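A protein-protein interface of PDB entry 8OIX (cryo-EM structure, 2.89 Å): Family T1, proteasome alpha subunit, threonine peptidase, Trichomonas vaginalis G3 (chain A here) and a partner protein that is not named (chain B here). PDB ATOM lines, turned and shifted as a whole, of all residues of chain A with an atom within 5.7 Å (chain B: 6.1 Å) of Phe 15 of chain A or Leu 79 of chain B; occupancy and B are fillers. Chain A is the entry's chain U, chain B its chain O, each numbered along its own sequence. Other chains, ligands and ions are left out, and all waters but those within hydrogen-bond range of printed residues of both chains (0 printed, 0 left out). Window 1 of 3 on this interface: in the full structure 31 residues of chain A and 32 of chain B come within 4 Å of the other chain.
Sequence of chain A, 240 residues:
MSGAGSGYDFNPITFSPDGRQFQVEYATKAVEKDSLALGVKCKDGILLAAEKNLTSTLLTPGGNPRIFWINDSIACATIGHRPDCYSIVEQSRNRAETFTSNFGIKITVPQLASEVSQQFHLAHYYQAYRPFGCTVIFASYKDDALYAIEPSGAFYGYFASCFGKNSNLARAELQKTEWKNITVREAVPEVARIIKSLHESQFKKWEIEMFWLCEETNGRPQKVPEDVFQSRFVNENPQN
OG1 of Thr 14 of chain A lies within hydrogen-bond range of O of Tyr 8 of chain B, 2.4 Å away.
The side-chain amide oxygen (OE1) of Gln 20 of chain B lies within hydrogen-bond range of the backbone NH (N) of Phe 15 of chain A (2.5 Å).
The side-chain amide oxygen (OE1) of Gln 30 of chain B sits close to the backbone carbonyl oxygen (O) of Gly 19 of chain A (3.3 Å).
NE2 of Gln 21 of chain A sits close to NE of Arg 128 of chain B.
NE of Arg 7 of chain B sits at hydrogen-bond distance from OH of Tyr 8 of chain B (3.1 Å).
The backbone carbonyl oxygen (O) of Arg 7 of chain B lies within hydrogen-bond range of the side-chain amide nitrogen (NE2) of Gln 20 of chain B, 2.4 Å away.
The backbone NH of Leu 79 of chain B sits at hydrogen-bond distance from the backbone carbonyl oxygen of Ala 131 of chain B, 3.2 Å away.
OD1 of Asp 82 of chain B lies within salt-bridge range of NH2 of Arg 128 of chain B (2.4 Å).
The side-chain carboxylate of Asp 82 of chain B sits at hydrogen-bond distance from the backbone NH of Ala 131 of chain B.
The side-chain hydroxyl (OG1) of Thr 14 of chain A sits close to the side-chain amide nitrogen (ND2) of Asn 11 of chain A (3.3 Å).
Among the printed residues, pairs that only touch across the chains: Ile 13 of chain A with Arg 128 of chain B, Tyr 8 of chain A with Arg 7 of chain B, Gln 21 of chain A with Leu 79 of chain B, Phe 15 of chain A with Tyr 23 of chain B, Phe 15 of chain A with Pro 129 of chain B, Arg 20 of chain A with Gln 30 of chain B, Gly 19 of chain A with Tyr 23 of chain B, Phe 15 of chain A with Arg 128 of chain B, Gly 19 of chain A with Ala 27 of chain B, Ser 16 of chain A with Tyr 23 of chain B, Tyr 8 of chain A with Tyr 8 of chain B, Thr 14 of chain A with Gln 20 of chain B, Phe 15 of chain A with Ala 27 of chain B, Pro 17 of chain A with Tyr 23 of chain B, Phe 15 of chain A with Ala 131 of chain B, Phe 15 of chain A with Leu 79 of chain B, Phe 15 of chain A with Ser 24 of chain B, Tyr 8 of chain A with Tyr 23 of chain B and Ile 13 of chain A with Gln 20 of chain B.
Of chain B, only Gln 20 (2.5 Å), Tyr 23 (3.2 Å), Ser 24 (3.7 Å), Ala 27 (3.5 Å), Leu 79 (3.6 Å), Arg 128 (3.3 Å), Pro 129 (3.2 Å) and Ala 131 (3.6 Å) come within 4 Å of Phe 15 of chain A.
Printed residues of chain B within 4 Å of Gln 21 of chain A: Leu 79 (3.2 Å) and Arg 128 (3.1 Å).
Of the printed residues of chain A, Ala 27 of chain B touches Phe 15 and Gly 19.
Val 28 of chain B touches none of the printed residues of chain A.
Ala 31 of chain B touches none of the printed residues of chain A.
Printed residues of chain A within 4 Å of Leu 79 of chain B: Phe 15 (3.6 Å) and Gln 21 (3.2 Å).
Printed residues of chain A within 4 Å of Arg 128 of chain B: Ile 13 (3.1 Å), Phe 15 (3.3 Å) and Gln 21 (3.1 Å).
The nearest residue of chain A that does not touch Leu 79 of chain B is Gly 19 of chain A (4.7 Å).
The nearest printed residue of chain A that does not touch Ser 24 of chain B is Gly 19 of chain A (5.4 Å).
Printed residues of chain B that touch a printed residue of chain A: Arg 7, Tyr 8, Gln 20, Tyr 23, Ser 24, Ala 27, Gln 30, Leu 79, Arg 128, Pro 129 and Ala 131.
Among the printed residues, no Asp or Glu carboxylate lies within 4 Å of a Lys or Arg side-chain nitrogen of the other chain.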
ATOM      1  N   TYR A   8     -30.052  16.624  17.590  1.00  0.00           N
ATOM      2  CA  TYR A   8     -29.354  16.067  18.742  1.00  0.00           C
ATOM      3  C   TYR A   8     -28.693  17.131  19.606  1.00  0.00           C
ATOM      4  O   TYR A   8     -27.965  16.783  20.542  1.00  0.00           O
ATOM      5  CB  TYR A   8     -28.304  15.056  18.273  1.00  0.00           C
ATOM      6  CG  TYR A   8     -28.879  13.899  17.489  1.00  0.00           C
ATOM      7  CD1 TYR A   8     -29.268  12.731  18.125  1.00  0.00           C
ATOM      8  CD2 TYR A   8     -29.051  13.984  16.114  1.00  0.00           C
ATOM      9  CE1 TYR A   8     -29.800  11.674  17.414  1.00  0.00           C
ATOM     10  CE2 TYR A   8     -29.584  12.934  15.395  1.00  0.00           C
ATOM     11  CZ  TYR A   8     -29.957  11.782  16.050  1.00  0.00           C
ATOM     12  OH  TYR A   8     -30.485  10.731  15.338  1.00  0.00           O
ATOM     13  N   ASN A  11     -31.137  18.529  23.690  1.00  0.00           N
ATOM     14  CA  ASN A  11     -31.132  17.854  24.978  1.00  0.00           C
ATOM     15  C   ASN A  11     -29.693  17.635  25.426  1.00  0.00           C
ATOM     16  O   ASN A  11     -28.912  17.035  24.677  1.00  0.00           O
ATOM     17  CB  ASN A  11     -31.865  16.529  24.878  1.00  0.00           C
ATOM     18  CG  ASN A  11     -32.164  15.916  26.229  1.00  0.00           C
ATOM     19  OD1 ASN A  11     -31.963  16.536  27.270  1.00  0.00           O
ATOM     20  ND2 ASN A  11     -32.670  14.691  26.214  1.00  0.00           N
ATOM     21  N   PRO A  12     -29.295  18.116  26.608  1.00  0.00           N
ATOM     22  CA  PRO A  12     -27.909  17.884  27.053  1.00  0.00           C
ATOM     23  C   PRO A  12     -27.542  16.416  27.156  1.00  0.00           C
ATOM     24  O   PRO A  12     -26.412  16.040  26.822  1.00  0.00           O
ATOM     25  CB  PRO A  12     -27.864  18.579  28.421  1.00  0.00           C
ATOM     26  CG  PRO A  12     -28.952  19.591  28.366  1.00  0.00           C
ATOM     27  CD  PRO A  12     -30.039  18.971  27.546  1.00  0.00           C
ATOM     28  N   ILE A  13     -28.469  15.568  27.608  1.00  0.00           N
ATOM     29  CA  ILE A  13     -28.167  14.149  27.777  1.00  0.00           C
ATOM     30  C   ILE A  13     -28.214  13.379  26.470  1.00  0.00           C
ATOM     31  O   ILE A  13     -27.873  12.191  26.451  1.00  0.00           O
ATOM     32  CB  ILE A  13     -29.127  13.500  28.789  1.00  0.00           C
ATOM     33  CG1 ILE A  13     -30.560  13.541  28.273  1.00  0.00           C
ATOM     34  CG2 ILE A  13     -29.050  14.221  30.113  1.00  0.00           C
ATOM     35  CD1 ILE A  13     -31.493  12.639  29.029  1.00  0.00           C
ATOM     36  N   THR A  14     -28.644  14.007  25.381  1.00  0.00           N
ATOM     37  CA  THR A  14     -28.739  13.316  24.106  1.00  0.00           C
ATOM     38  C   THR A  14     -27.357  13.191  23.480  1.00  0.00           C
ATOM     39  O   THR A  14     -26.554  14.127  23.518  1.00  0.00           O
ATOM     40  CB  THR A  14     -29.692  14.061  23.168  1.00  0.00           C
ATOM     41  OG1 THR A  14     -31.045  13.770  23.536  1.00  0.00           O
ATOM     42  CG2 THR A  14     -29.475  13.653  21.718  1.00  0.00           C
ATOM     43  N   PHE A  15     -27.083  12.024  22.906  1.00  0.00           N
ATOM     44  CA  PHE A  15     -25.842  11.771  22.192  1.00  0.00           C
ATOM     45  C   PHE A  15     -26.070  11.929  20.697  1.00  0.00           C
ATOM     46  O   PHE A  15     -27.056  11.418  20.156  1.00  0.00           O
ATOM     47  CB  PHE A  15     -25.317  10.366  22.481  1.00  0.00           C
ATOM     48  CG  PHE A  15     -24.364  10.288  23.634  1.00  0.00           C
ATOM     49  CD1 PHE A  15     -23.188  11.013  23.626  1.00  0.00           C
ATOM     50  CD2 PHE A  15     -24.623   9.453  24.704  1.00  0.00           C
ATOM     51  CE1 PHE A  15     -22.305  10.929  24.678  1.00  0.00           C
ATOM     52  CE2 PHE A  15     -23.740   9.364  25.756  1.00  0.00           C
ATOM     53  CZ  PHE A  15     -22.580  10.106  25.744  1.00  0.00           C
ATOM     54  N   SER A  16     -25.164  12.641  20.037  1.00  0.00           N
ATOM     55  CA  SER A  16     -25.175  12.698  18.589  1.00  0.00           C
ATOM     56  C   SER A  16     -24.823  11.325  18.019  1.00  0.00           C
ATOM     57  O   SER A  16     -24.123  10.540  18.663  1.00  0.00           O
ATOM     58  CB  SER A  16     -24.179  13.742  18.093  1.00  0.00           C
ATOM     59  OG  SER A  16     -24.108  13.771  16.679  1.00  0.00           O
ATOM     60  N   PRO A  17     -25.311  11.002  16.816  1.00  0.00           N
ATOM     61  CA  PRO A  17     -24.938   9.722  16.193  1.00  0.00           C
ATOM     62  C   PRO A  17     -23.438   9.520  16.047  1.00  0.00           C
ATOM     63  O   PRO A  17     -23.014   8.396  15.756  1.00  0.00           O
ATOM     64  CB  PRO A  17     -25.630   9.784  14.828  1.00  0.00           C
ATOM     65  CG  PRO A  17     -26.811  10.649  15.067  1.00  0.00           C
ATOM     66  CD  PRO A  17     -26.366  11.691  16.055  1.00  0.00           C
ATOM     67  N   GLY A  19     -21.569  10.263  18.703  1.00  0.00           N
ATOM     68  CA  GLY A  19     -21.179  10.272  20.098  1.00  0.00           C
ATOM     69  C   GLY A  19     -20.883  11.638  20.669  1.00  0.00           C
ATOM     70  O   GLY A  19     -20.406  11.726  21.805  1.00  0.00           O
ATOM     71  N   ARG A  20     -21.148  12.704  19.921  1.00  0.00           N
ATOM     72  CA  ARG A  20     -20.887  14.054  20.393  1.00  0.00           C
ATOM     73  C   ARG A  20     -22.006  14.534  21.307  1.00  0.00           C
ATOM     74  O   ARG A  20     -23.185  14.267  21.064  1.00  0.00           O
ATOM     75  CB  ARG A  20     -20.742  15.011  19.210  1.00  0.00           C
ATOM     76  CG  ARG A  20     -19.697  14.587  18.197  1.00  0.00           C
ATOM     77  CD  ARG A  20     -19.731  15.471  16.964  1.00  0.00           C
ATOM     78  NE  ARG A  20     -19.441  16.864  17.278  1.00  0.00           N
ATOM     79  CZ  ARG A  20     -19.532  17.860  16.409  1.00  0.00           C
ATOM     80  NH1 ARG A  20     -19.925  17.656  15.163  1.00  0.00           N
ATOM     81  NH2 ARG A  20     -19.228  19.094  16.802  1.00  0.00           N
ATOM     82  N   GLN A  21     -21.628  15.237  22.370  1.00  0.00           N
ATOM     83  CA  GLN A  21     -22.585  15.884  23.264  1.00  0.00           C
ATOM     84  C   GLN A  21     -22.672  17.341  22.832  1.00  0.00           C
ATOM     85  O   GLN A  21     -21.882  18.185  23.259  1.00  0.00           O
ATOM     86  CB  GLN A  21     -22.168  15.753  24.722  1.00  0.00           C
ATOM     87  CG  GLN A  21     -21.843  14.347  25.162  1.00  0.00           C
ATOM     88  CD  GLN A  21     -21.836  14.217  26.665  1.00  0.00           C
ATOM     89  OE1 GLN A  21     -20.788  14.032  27.281  1.00  0.00           O
ATOM     90  NE2 GLN A  21     -23.012  14.319  27.271  1.00  0.00           N
ATOM     91  N   ARG B   7     -34.503   8.491  18.848  1.00  0.00           N
ATOM     92  CA  ARG B   7     -33.135   8.824  18.481  1.00  0.00           C
ATOM     93  C   ARG B   7     -32.478   9.801  19.443  1.00  0.00           C
ATOM     94  O   ARG B   7     -31.246   9.834  19.522  1.00  0.00           O
ATOM     95  CB  ARG B   7     -33.098   9.399  17.060  1.00  0.00           C
ATOM     96  CG  ARG B   7     -34.187  10.416  16.777  1.00  0.00           C
ATOM     97  CD  ARG B   7     -34.156  10.873  15.330  1.00  0.00           C
ATOM     98  NE  ARG B   7     -35.097  11.960  15.088  1.00  0.00           N
ATOM     99  CZ  ARG B   7     -36.369  11.792  14.753  1.00  0.00           C
ATOM    100  NH1 ARG B   7     -36.891  10.585  14.604  1.00  0.00           N
ATOM    101  NH2 ARG B   7     -37.138  12.861  14.568  1.00  0.00           N
ATOM    102  N   TYR B   8     -33.266  10.582  20.180  1.00  0.00           N
ATOM    103  CA  TYR B   8     -32.736  11.566  21.112  1.00  0.00           C
ATOM    104  C   TYR B   8     -32.808  11.113  22.561  1.00  0.00           C
ATOM    105  O   TYR B   8     -32.005  11.568  23.381  1.00  0.00           O
ATOM    106  CB  TYR B   8     -33.489  12.890  20.956  1.00  0.00           C
ATOM    107  CG  TYR B   8     -33.541  13.368  19.525  1.00  0.00           C
ATOM    108  CD1 TYR B   8     -32.381  13.674  18.835  1.00  0.00           C
ATOM    109  CD2 TYR B   8     -34.750  13.500  18.860  1.00  0.00           C
ATOM    110  CE1 TYR B   8     -32.422  14.101  17.527  1.00  0.00           C
ATOM    111  CE2 TYR B   8     -34.802  13.934  17.553  1.00  0.00           C
ATOM    112  CZ  TYR B   8     -33.633  14.232  16.890  1.00  0.00           C
ATOM    113  OH  TYR B   8     -33.676  14.662  15.584  1.00  0.00           O
ATOM    114  N   TRP B  19     -30.913   3.827  20.168  1.00  0.00           N
ATOM    115  CA  TRP B  19     -29.949   4.619  19.412  1.00  0.00           C
ATOM    116  C   TRP B  19     -28.995   5.364  20.333  1.00  0.00           C
ATOM    117  O   TRP B  19     -27.804   5.497  20.028  1.00  0.00           O
ATOM    118  CB  TRP B  19     -30.682   5.588  18.490  1.00  0.00           C
ATOM    119  CG  TRP B  19     -31.234   4.920  17.277  1.00  0.00           C
ATOM    120  CD1 TRP B  19     -32.547   4.797  16.937  1.00  0.00           C
ATOM    121  CD2 TRP B  19     -30.488   4.263  16.247  1.00  0.00           C
ATOM    122  NE1 TRP B  19     -32.667   4.112  15.753  1.00  0.00           N
ATOM    123  CE2 TRP B  19     -31.416   3.773  15.309  1.00  0.00           C
ATOM    124  CE3 TRP B  19     -29.125   4.048  16.023  1.00  0.00           C
ATOM    125  CZ2 TRP B  19     -31.026   3.080  14.167  1.00  0.00           C
ATOM    126  CZ3 TRP B  19     -28.741   3.360  14.890  1.00  0.00           C
ATOM    127  CH2 TRP B  19     -29.686   2.884  13.975  1.00  0.00           C
ATOM    128  N   GLN B  20     -29.494   5.848  21.471  1.00  0.00           N
ATOM    129  CA  GLN B  20     -28.635   6.569  22.404  1.00  0.00           C
ATOM    130  C   GLN B  20     -27.556   5.661  22.975  1.00  0.00           C
ATOM    131  O   GLN B  20     -26.437   6.109  23.238  1.00  0.00           O
ATOM    132  CB  GLN B  20     -29.471   7.186  23.521  1.00  0.00           C
ATOM    133  CG  GLN B  20     -30.292   8.371  23.069  1.00  0.00           C
ATOM    134  CD  GLN B  20     -29.431   9.508  22.568  1.00  0.00           C
ATOM    135  OE1 GLN B  20     -28.562  10.005  23.281  1.00  0.00           O
ATOM    136  NE2 GLN B  20     -29.666   9.927  21.332  1.00  0.00           N
ATOM    137  N   TYR B  23     -24.926   5.358  20.376  1.00  0.00           N
ATOM    138  CA  TYR B  23     -24.195   6.613  20.298  1.00  0.00           C
ATOM    139  C   TYR B  23     -23.271   6.783  21.495  1.00  0.00           C
ATOM    140  O   TYR B  23     -22.215   7.408  21.375  1.00  0.00           O
ATOM    141  CB  TYR B  23     -25.174   7.780  20.187  1.00  0.00           C
ATOM    142  CG  TYR B  23     -26.128   7.690  19.014  1.00  0.00           C
ATOM    143  CD1 TYR B  23     -25.877   6.837  17.945  1.00  0.00           C
ATOM    144  CD2 TYR B  23     -27.290   8.449  18.982  1.00  0.00           C
ATOM    145  CE1 TYR B  23     -26.749   6.750  16.881  1.00  0.00           C
ATOM    146  CE2 TYR B  23     -28.168   8.368  17.920  1.00  0.00           C
ATOM    147  CZ  TYR B  23     -27.891   7.517  16.872  1.00  0.00           C
ATOM    148  OH  TYR B  23     -28.761   7.430  15.810  1.00  0.00           O
ATOM    149  N   SER B  24     -23.642   6.236  22.656  1.00  0.00           N
ATOM    150  CA  SER B  24     -22.710   6.193  23.779  1.00  0.00           C
ATOM    151  C   SER B  24     -21.530   5.276  23.484  1.00  0.00           C
ATOM    152  O   SER B  24     -20.409   5.544  23.928  1.00  0.00           O
ATOM    153  CB  SER B  24     -23.430   5.743  25.049  1.00  0.00           C
ATOM    154  OG  SER B  24     -24.009   4.463  24.879  1.00  0.00           O
ATOM    155  N   ALA B  27     -19.382   7.401  21.506  1.00  0.00           N
ATOM    156  CA  ALA B  27     -18.736   8.345  22.412  1.00  0.00           C
ATOM    157  C   ALA B  27     -17.561   7.697  23.136  1.00  0.00           C
ATOM    158  O   ALA B  27     -16.547   8.353  23.402  1.00  0.00           O
ATOM    159  CB  ALA B  27     -19.750   8.897  23.408  1.00  0.00           C
ATOM    160  N   VAL B  28     -17.688   6.415  23.481  1.00  0.00           N
ATOM    161  CA  VAL B  28     -16.545   5.674  24.012  1.00  0.00           C
ATOM    162  C   VAL B  28     -15.429   5.639  22.980  1.00  0.00           C
ATOM    163  O   VAL B  28     -14.252   5.846  23.299  1.00  0.00           O
ATOM    164  CB  VAL B  28     -16.964   4.253  24.426  1.00  0.00           C
ATOM    165  CG1 VAL B  28     -15.739   3.416  24.750  1.00  0.00           C
ATOM    166  CG2 VAL B  28     -17.875   4.312  25.611  1.00  0.00           C
ATOM    167  N   GLN B  30     -14.862   7.845  20.966  1.00  0.00           N
ATOM    168  CA  GLN B  30     -14.316   9.199  20.950  1.00  0.00           C
ATOM    169  C   GLN B  30     -13.223   9.425  21.988  1.00  0.00           C
ATOM    170  O   GLN B  30     -12.638  10.513  22.004  1.00  0.00           O
ATOM    171  CB  GLN B  30     -15.428  10.226  21.168  1.00  0.00           C
ATOM    172  CG  GLN B  30     -16.278  10.499  19.949  1.00  0.00           C
ATOM    173  CD  GLN B  30     -17.004  11.821  20.050  1.00  0.00           C
ATOM    174  OE1 GLN B  30     -17.267  12.314  21.147  1.00  0.00           O
ATOM    175  NE2 GLN B  30     -17.324  12.408  18.904  1.00  0.00           N
ATOM    176  N   ALA B  31     -12.936   8.451  22.854  1.00  0.00           N
ATOM    177  CA  ALA B  31     -11.886   8.619  23.853  1.00  0.00           C
ATOM    178  C   ALA B  31     -10.491   8.704  23.248  1.00  0.00           C
ATOM    179  O   ALA B  31      -9.555   9.083  23.960  1.00  0.00           O
ATOM    180  CB  ALA B  31     -11.935   7.476  24.867  1.00  0.00           C
ATOM    181  N   VAL B  77     -12.534   3.366  29.500  1.00  0.00           N
ATOM    182  CA  VAL B  77     -12.328   4.069  28.240  1.00  0.00           C
ATOM    183  C   VAL B  77     -13.639   4.734  27.858  1.00  0.00           C
ATOM    184  O   VAL B  77     -14.668   4.064  27.720  1.00  0.00           O
ATOM    185  CB  VAL B  77     -11.843   3.121  27.134  1.00  0.00           C
ATOM    186  CG1 VAL B  77     -11.739   3.861  25.813  1.00  0.00           C
ATOM    187  CG2 VAL B  77     -10.507   2.513  27.514  1.00  0.00           C
ATOM    188  N   GLY B  78     -13.609   6.049  27.683  1.00  0.00           N
ATOM    189  CA  GLY B  78     -14.814   6.765  27.315  1.00  0.00           C
ATOM    190  C   GLY B  78     -14.620   8.255  27.491  1.00  0.00           C
ATOM    191  O   GLY B  78     -13.491   8.738  27.584  1.00  0.00           O
ATOM    192  N   LEU B  79     -15.737   8.967  27.522  1.00  0.00           N
ATOM    193  CA  LEU B  79     -15.690  10.401  27.753  1.00  0.00           C
ATOM    194  C   LEU B  79     -15.067  10.672  29.119  1.00  0.00           C
ATOM    195  O   LEU B  79     -15.483  10.063  30.114  1.00  0.00           O
ATOM    196  CB  LEU B  79     -17.091  11.001  27.675  1.00  0.00           C
ATOM    197  CG  LEU B  79     -17.857  10.699  26.388  1.00  0.00           C
ATOM    198  CD1 LEU B  79     -19.119  11.525  26.317  1.00  0.00           C
ATOM    199  CD2 LEU B  79     -16.983  10.971  25.178  1.00  0.00           C
ATOM    200  N   PRO B  80     -14.072  11.559  29.209  1.00  0.00           N
ATOM    201  CA  PRO B  80     -13.375  11.749  30.493  1.00  0.00           C
ATOM    202  C   PRO B  80     -14.300  12.129  31.633  1.00  0.00           C
ATOM    203  O   PRO B  80     -14.102  11.675  32.766  1.00  0.00           O
ATOM    204  CB  PRO B  80     -12.368  12.864  30.179  1.00  0.00           C
ATOM    205  CG  PRO B  80     -12.219  12.845  28.692  1.00  0.00           C
ATOM    206  CD  PRO B  80     -13.539  12.424  28.146  1.00  0.00           C
ATOM    207  N   SER B  81     -15.312  12.953  31.360  1.00  0.00           N
ATOM    208  CA  SER B  81     -16.309  13.263  32.377  1.00  0.00           C
ATOM    209  C   SER B  81     -17.076  12.014  32.783  1.00  0.00           C
ATOM    210  O   SER B  81     -17.284  11.755  33.975  1.00  0.00           O
ATOM    211  CB  SER B  81     -17.267  14.323  31.851  1.00  0.00           C
ATOM    212  OG  SER B  81     -17.823  13.930  30.608  1.00  0.00           O
ATOM    213  N   ASP B  82     -17.505  11.226  31.797  1.00  0.00           N
ATOM    214  CA  ASP B  82     -18.189   9.979  32.101  1.00  0.00           C
ATOM    215  C   ASP B  82     -17.252   9.007  32.799  1.00  0.00           C
ATOM    216  O   ASP B  82     -17.680   8.245  33.668  1.00  0.00           O
ATOM    217  CB  ASP B  82     -18.758   9.360  30.824  1.00  0.00           C
ATOM    218  CG  ASP B  82     -19.993  10.078  30.328  1.00  0.00           C
ATOM    219  OD1 ASP B  82     -20.797  10.528  31.167  1.00  0.00           O
ATOM    220  OD2 ASP B  82     -20.167  10.189  29.097  1.00  0.00           O
ATOM    221  N   VAL B  83     -15.969   9.020  32.435  1.00  0.00           N
ATOM    222  CA  VAL B  83     -15.003   8.148  33.097  1.00  0.00           C
ATOM    223  C   VAL B  83     -14.872   8.514  34.570  1.00  0.00           C
ATOM    224  O   VAL B  83     -14.836   7.637  35.437  1.00  0.00           O
ATOM    225  CB  VAL B  83     -13.646   8.203  32.373  1.00  0.00           C
ATOM    226  CG1 VAL B  83     -12.574   7.537  33.210  1.00  0.00           C
ATOM    227  CG2 VAL B  83     -13.746   7.527  31.021  1.00  0.00           C
ATOM    228  N   ASN B  84     -14.794   9.809  34.879  1.00  0.00           N
ATOM    229  CA  ASN B  84     -14.722  10.228  36.277  1.00  0.00           C
ATOM    230  C   ASN B  84     -16.014   9.907  37.021  1.00  0.00           C
ATOM    231  O   ASN B  84     -15.983   9.482  38.185  1.00  0.00           O
ATOM    232  CB  ASN B  84     -14.399  11.718  36.364  1.00  0.00           C
ATOM    233  CG  ASN B  84     -13.076  12.062  35.711  1.00  0.00           C
ATOM    234  OD1 ASN B  84     -12.012  11.700  36.214  1.00  0.00           O
ATOM    235  ND2 ASN B  84     -13.133  12.769  34.590  1.00  0.00           N
ATOM    236  N   ARG B 128     -28.618  10.031  30.786  1.00  0.00           N
ATOM    237  CA  ARG B 128     -27.797   9.709  29.634  1.00  0.00           C
ATOM    238  C   ARG B 128     -27.083   8.379  29.854  1.00  0.00           C
ATOM    239  O   ARG B 128     -26.569   8.125  30.946  1.00  0.00           O
ATOM    240  CB  ARG B 128     -26.772  10.812  29.391  1.00  0.00           C
ATOM    241  CG  ARG B 128     -25.898  10.580  28.181  1.00  0.00           C
ATOM    242  CD  ARG B 128     -25.033  11.789  27.901  1.00  0.00           C
ATOM    243  NE  ARG B 128     -24.287  12.212  29.078  1.00  0.00           N
ATOM    244  CZ  ARG B 128     -23.238  11.568  29.570  1.00  0.00           C
ATOM    245  NH1 ARG B 128     -22.793  10.450  29.023  1.00  0.00           N
ATOM    246  NH2 ARG B 128     -22.621  12.058  30.640  1.00  0.00           N
ATOM    247  N   PRO B 129     -27.052   7.502  28.852  1.00  0.00           N
ATOM    248  CA  PRO B 129     -26.178   6.324  28.939  1.00  0.00           C
ATOM    249  C   PRO B 129     -24.734   6.754  29.135  1.00  0.00           C
ATOM    250  O   PRO B 129     -24.158   7.454  28.298  1.00  0.00           O
ATOM    251  CB  PRO B 129     -26.390   5.627  27.591  1.00  0.00           C
ATOM    252  CG  PRO B 129     -27.728   6.090  27.135  1.00  0.00           C
ATOM    253  CD  PRO B 129     -27.865   7.498  27.625  1.00  0.00           C
ATOM    254  N   SER B 130     -24.149   6.338  30.256  1.00  0.00           N
ATOM    255  CA  SER B 130     -22.785   6.738  30.586  1.00  0.00           C
ATOM    256  C   SER B 130     -21.826   6.097  29.594  1.00  0.00           C
ATOM    257  O   SER B 130     -21.655   4.874  29.580  1.00  0.00           O
ATOM    258  CB  SER B 130     -22.443   6.341  32.018  1.00  0.00           C
ATOM    259  OG  SER B 130     -21.344   7.088  32.501  1.00  0.00           O
ATOM    260  N   ALA B 131     -21.198   6.927  28.762  1.00  0.00           N
ATOM    261  CA  ALA B 131     -20.354   6.454  27.666  1.00  0.00           C
ATOM    262  C   ALA B 131     -18.983   6.048  28.205  1.00  0.00           C
ATOM    263  O   ALA B 131     -17.970   6.722  28.012  1.00  0.00           O
ATOM    264  CB  ALA B 131     -20.235   7.523  26.593  1.00  0.00           C
ATOM    265  N   VAL B 132     -18.963   4.907  28.892  1.00  0.00           N
ATOM    266  CA  VAL B 132     -17.735   4.352  29.451  1.00  0.00           C
ATOM    267  C   VAL B 132     -17.751   2.843  29.268  1.00  0.00           C
ATOM    268  O   VAL B 132     -18.599   2.153  29.845  1.00  0.00           O
ATOM    269  CB  VAL B 132     -17.555   4.694  30.939  1.00  0.00           C
ATOM    270  CG1 VAL B 132     -16.402   3.899  31.524  1.00  0.00           C
ATOM    271  CG2 VAL B 132     -17.291   6.158  31.105  1.00  0.00           C
